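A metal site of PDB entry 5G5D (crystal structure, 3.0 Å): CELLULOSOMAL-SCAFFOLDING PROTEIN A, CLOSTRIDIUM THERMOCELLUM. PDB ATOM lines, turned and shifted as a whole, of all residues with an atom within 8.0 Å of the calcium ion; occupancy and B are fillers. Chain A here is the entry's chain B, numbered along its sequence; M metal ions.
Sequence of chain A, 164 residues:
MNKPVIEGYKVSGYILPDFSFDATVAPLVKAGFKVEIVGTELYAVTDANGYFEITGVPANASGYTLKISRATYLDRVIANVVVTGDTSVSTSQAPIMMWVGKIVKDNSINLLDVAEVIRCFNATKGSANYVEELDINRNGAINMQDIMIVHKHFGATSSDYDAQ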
ATOM      1  N   THR A  72     -28.393  22.836  19.462  1.00  0.00           N
ATOM      2  CA  THR A  72     -27.129  22.190  19.069  1.00  0.00           C
ATOM      3  C   THR A  72     -27.265  20.852  18.321  1.00  0.00           C
ATOM      4  O   THR A  72     -26.275  20.385  17.756  1.00  0.00           O
ATOM      5  CB  THR A  72     -26.101  22.029  20.223  1.00  0.00           C
ATOM      6  OG1 THR A  72     -26.438  20.912  21.060  1.00  0.00           O
ATOM      7  CG2 THR A  72     -25.985  23.307  21.061  1.00  0.00           C
ATOM      8  N   LEU A  74     -28.987  18.032  15.429  1.00  0.00           N
ATOM      9  CA  LEU A  74     -29.512  17.941  14.070  1.00  0.00           C
ATOM     10  C   LEU A  74     -30.923  17.346  14.140  1.00  0.00           C
ATOM     11  O   LEU A  74     -31.086  16.131  14.287  1.00  0.00           O
ATOM     12  CB  LEU A  74     -28.573  17.114  13.174  1.00  0.00           C
ATOM     13  CG  LEU A  74     -28.976  16.604  11.771  1.00  0.00           C
ATOM     14  CD1 LEU A  74     -29.566  17.669  10.857  1.00  0.00           C
ATOM     15  CD2 LEU A  74     -27.771  15.963  11.084  1.00  0.00           C
ATOM     16  N   GLY A 101     -24.542  18.483  16.476  1.00  0.00           N
ATOM     17  CA  GLY A 101     -23.822  19.044  15.336  1.00  0.00           C
ATOM     18  C   GLY A 101     -24.348  20.333  14.710  1.00  0.00           C
ATOM     19  O   GLY A 101     -23.555  21.093  14.181  1.00  0.00           O
ATOM     20  N   LYS A 102     -25.662  20.563  14.737  1.00  0.00           N
ATOM     21  CA  LYS A 102     -26.233  21.827  14.241  1.00  0.00           C
ATOM     22  C   LYS A 102     -26.257  22.876  15.338  1.00  0.00           C
ATOM     23  O   LYS A 102     -27.270  23.064  16.002  1.00  0.00           O
ATOM     24  CB  LYS A 102     -27.643  21.625  13.695  1.00  0.00           C
ATOM     25  CG  LYS A 102     -27.761  21.663  12.186  1.00  0.00           C
ATOM     26  CD  LYS A 102     -29.000  20.932  11.731  1.00  0.00           C
ATOM     27  CE  LYS A 102     -30.289  21.514  12.315  1.00  0.00           C
ATOM     28  NZ  LYS A 102     -31.550  20.858  11.860  1.00  0.00           N
ATOM     29  N   ILE A 103     -25.132  23.567  15.499  1.00  0.00           N
ATOM     30  CA  ILE A 103     -25.057  24.707  16.419  1.00  0.00           C
ATOM     31  C   ILE A 103     -25.622  25.911  15.650  1.00  0.00           C
ATOM     32  O   ILE A 103     -26.464  26.649  16.171  1.00  0.00           O
ATOM     33  CB  ILE A 103     -23.615  24.945  16.931  1.00  0.00           C
ATOM     34  CG1 ILE A 103     -23.180  23.817  17.887  1.00  0.00           C
ATOM     35  CG2 ILE A 103     -23.511  26.268  17.677  1.00  0.00           C
ATOM     36  CD1 ILE A 103     -22.885  22.487  17.226  1.00  0.00           C
ATOM     37  N   VAL A 104     -25.163  26.084  14.407  1.00  0.00           N
ATOM     38  CA  VAL A 104     -25.796  26.979  13.444  1.00  0.00           C
ATOM     39  C   VAL A 104     -26.925  26.191  12.776  1.00  0.00           C
ATOM     40  O   VAL A 104     -26.661  25.344  11.923  1.00  0.00           O
ATOM     41  CB  VAL A 104     -24.785  27.476  12.379  1.00  0.00           C
ATOM     42  CG1 VAL A 104     -25.466  28.405  11.385  1.00  0.00           C
ATOM     43  CG2 VAL A 104     -23.604  28.185  13.047  1.00  0.00           C
ATOM     44  N   LYS A 105     -28.169  26.460  13.170  1.00  0.00           N
ATOM     45  CA  LYS A 105     -29.333  25.724  12.650  1.00  0.00           C
ATOM     46  C   LYS A 105     -29.617  26.064  11.179  1.00  0.00           C
ATOM     47  O   LYS A 105     -30.231  27.092  10.874  1.00  0.00           O
ATOM     48  CB  LYS A 105     -30.588  25.995  13.487  1.00  0.00           C
ATOM     49  CG  LYS A 105     -30.553  25.439  14.906  1.00  0.00           C
ATOM     50  CD  LYS A 105     -30.893  23.947  14.963  1.00  0.00           C
ATOM     51  CE  LYS A 105     -30.857  23.399  16.394  1.00  0.00           C
ATOM     52  NZ  LYS A 105     -32.016  23.813  17.231  1.00  0.00           N
ATOM     53  N   ASP A 106     -29.126  25.212  10.274  1.00  0.00           N
ATOM     54  CA  ASP A 106     -29.420  25.339   8.835  1.00  0.00           C
ATOM     55  C   ASP A 106     -29.666  23.983   8.128  1.00  0.00           C
ATOM     56  O   ASP A 106     -29.606  23.917   6.884  1.00  0.00           O
ATOM     57  CB  ASP A 106     -28.310  26.148   8.150  1.00  0.00           C
ATOM     58  CG  ASP A 106     -26.909  25.610   8.416  1.00  0.00           C
ATOM     59  OD1 ASP A 106     -26.718  24.380   8.442  1.00  0.00           O
ATOM     60  OD2 ASP A 106     -25.981  26.423   8.604  1.00  0.00           O
ATOM     61  N   ASN A 107     -29.988  22.949   8.912  1.00  0.00           N
ATOM     62  CA  ASN A 107     -30.150  21.569   8.443  1.00  0.00           C
ATOM     63  C   ASN A 107     -28.889  20.962   7.802  1.00  0.00           C
ATOM     64  O   ASN A 107     -28.962  20.269   6.784  1.00  0.00           O
ATOM     65  CB  ASN A 107     -31.367  21.430   7.523  1.00  0.00           C
ATOM     66  CG  ASN A 107     -31.819  19.988   7.339  1.00  0.00           C
ATOM     67  OD1 ASN A 107     -31.458  19.117   8.123  1.00  0.00           O
ATOM     68  ND2 ASN A 107     -32.582  19.742   6.282  1.00  0.00           N
ATOM     69  N   SER A 108     -27.740  21.237   8.397  1.00  0.00           N
ATOM     70  CA  SER A 108     -26.474  20.616   7.990  1.00  0.00           C
ATOM     71  C   SER A 108     -25.426  20.752   9.102  1.00  0.00           C
ATOM     72  O   SER A 108     -25.483  21.678   9.903  1.00  0.00           O
ATOM     73  CB  SER A 108     -25.946  21.257   6.702  1.00  0.00           C
ATOM     74  OG  SER A 108     -24.678  20.729   6.338  1.00  0.00           O
ATOM     75  N   ILE A 109     -24.489  19.811   9.125  1.00  0.00           N
ATOM     76  CA  ILE A 109     -23.304  19.887   9.980  1.00  0.00           C
ATOM     77  C   ILE A 109     -22.135  20.254   9.073  1.00  0.00           C
ATOM     78  O   ILE A 109     -21.797  19.486   8.154  1.00  0.00           O
ATOM     79  CB  ILE A 109     -23.060  18.582  10.778  1.00  0.00           C
ATOM     80  CG1 ILE A 109     -24.268  18.312  11.689  1.00  0.00           C
ATOM     81  CG2 ILE A 109     -21.792  18.694  11.607  1.00  0.00           C
ATOM     82  CD1 ILE A 109     -24.321  16.951  12.353  1.00  0.00           C
ATOM     83  N   ASN A 110     -21.529  21.419   9.297  1.00  0.00           N
ATOM     84  CA  ASN A 110     -20.473  21.936   8.431  1.00  0.00           C
ATOM     85  C   ASN A 110     -19.450  22.798   9.193  1.00  0.00           C
ATOM     86  O   ASN A 110     -19.516  22.922  10.419  1.00  0.00           O
ATOM     87  CB  ASN A 110     -21.087  22.689   7.227  1.00  0.00           C
ATOM     88  CG  ASN A 110     -22.195  23.656   7.618  1.00  0.00           C
ATOM     89  OD1 ASN A 110     -22.014  24.490   8.511  1.00  0.00           O
ATOM     90  ND2 ASN A 110     -23.318  23.587   6.927  1.00  0.00           N
ATOM     91  N   LEU A 111     -18.475  23.326   8.456  1.00  0.00           N
ATOM     92  CA  LEU A 111     -17.460  24.271   8.961  1.00  0.00           C
ATOM     93  C   LEU A 111     -17.956  25.279   9.995  1.00  0.00           C
ATOM     94  O   LEU A 111     -17.299  25.495  11.019  1.00  0.00           O
ATOM     95  CB  LEU A 111     -16.871  25.045   7.774  1.00  0.00           C
ATOM     96  CG  LEU A 111     -15.845  26.142   8.067  1.00  0.00           C
ATOM     97  CD1 LEU A 111     -14.566  25.512   8.615  1.00  0.00           C
ATOM     98  CD2 LEU A 111     -15.570  26.942   6.807  1.00  0.00           C
ATOM     99  N   LEU A 112     -19.098  25.891   9.716  1.00  0.00           N
ATOM    100  CA  LEU A 112     -19.684  26.924  10.565  1.00  0.00           C
ATOM    101  C   LEU A 112     -19.996  26.423  11.980  1.00  0.00           C
ATOM    102  O   LEU A 112     -19.791  27.138  12.967  1.00  0.00           O
ATOM    103  CB  LEU A 112     -20.953  27.510   9.934  1.00  0.00           C
ATOM    104  CG  LEU A 112     -20.849  28.202   8.563  1.00  0.00           C
ATOM    105  CD1 LEU A 112     -22.157  28.900   8.228  1.00  0.00           C
ATOM    106  CD2 LEU A 112     -19.697  29.190   8.506  1.00  0.00           C
ATOM    107  N   ASP A 113     -20.469  25.177  12.071  1.00  0.00           N
ATOM    108  CA  ASP A 113     -20.775  24.542  13.351  1.00  0.00           C
ATOM    109  C   ASP A 113     -19.504  24.239  14.142  1.00  0.00           C
ATOM    110  O   ASP A 113     -19.461  24.433  15.361  1.00  0.00           O
ATOM    111  CB  ASP A 113     -21.518  23.228  13.128  1.00  0.00           C
ATOM    112  CG  ASP A 113     -22.852  23.430  12.449  1.00  0.00           C
ATOM    113  OD1 ASP A 113     -23.753  24.030  13.063  1.00  0.00           O
ATOM    114  OD2 ASP A 113     -23.017  22.999  11.292  1.00  0.00           O
ATOM    115  N   VAL A 114     -18.485  23.759  13.440  1.00  0.00           N
ATOM    116  CA  VAL A 114     -17.198  23.432  14.060  1.00  0.00           C
ATOM    117  C   VAL A 114     -16.597  24.715  14.621  1.00  0.00           C
ATOM    118  O   VAL A 114     -16.087  24.716  15.753  1.00  0.00           O
ATOM    119  CB  VAL A 114     -16.229  22.768  13.067  1.00  0.00           C
ATOM    120  CG1 VAL A 114     -14.986  22.259  13.779  1.00  0.00           C
ATOM    121  CG2 VAL A 114     -16.889  21.608  12.322  1.00  0.00           C
ATOM    122  N   ALA A 156     -23.842  15.788   7.586  1.00  0.00           N
ATOM    123  CA  ALA A 156     -25.086  15.066   7.793  1.00  0.00           C
ATOM    124  C   ALA A 156     -26.279  16.011   7.709  1.00  0.00           C
ATOM    125  O   ALA A 156     -26.253  17.074   8.324  1.00  0.00           O
ATOM    126  CB  ALA A 156     -25.072  14.363   9.147  1.00  0.00           C
HETATM  127 CA    CA M   1     -25.320  23.899  10.667  1.00  0.00          CA
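The side-chain hydroxyl (OG) of Ser 108 sits at hydrogen-bond distance from the side-chain amide nitrogen (ND2) of Asn 110 (3.2 Å).
The backbone NH (N) of Asn 110 sits close to the side-chain carboxylate (OD2) of Asp 113 (2.9 Å).
OD1 of Asn 110 lies close to N of Leu 112 (3.5 Å).
N of Lys 102 lies within hydrogen-bond range of O of Thr 72 (3.1 Å).
N of Ile 103 sits close to OD1 of Asp 113.
Lys 102 touches the calcium ion.
OD1 of Asn 110 touches the calcium ion, at 3.99 Å.
Within 4 Å of the calcium ion: Lys 102, Val 104, Asp 106, Ser 108, Asn 110 and Asp 113.
The calcium ion is bound by O of Val 104, O of Ser 108, OD2 of Asp 113, OD1 of Asp 106 and OD1 of Asp 113.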
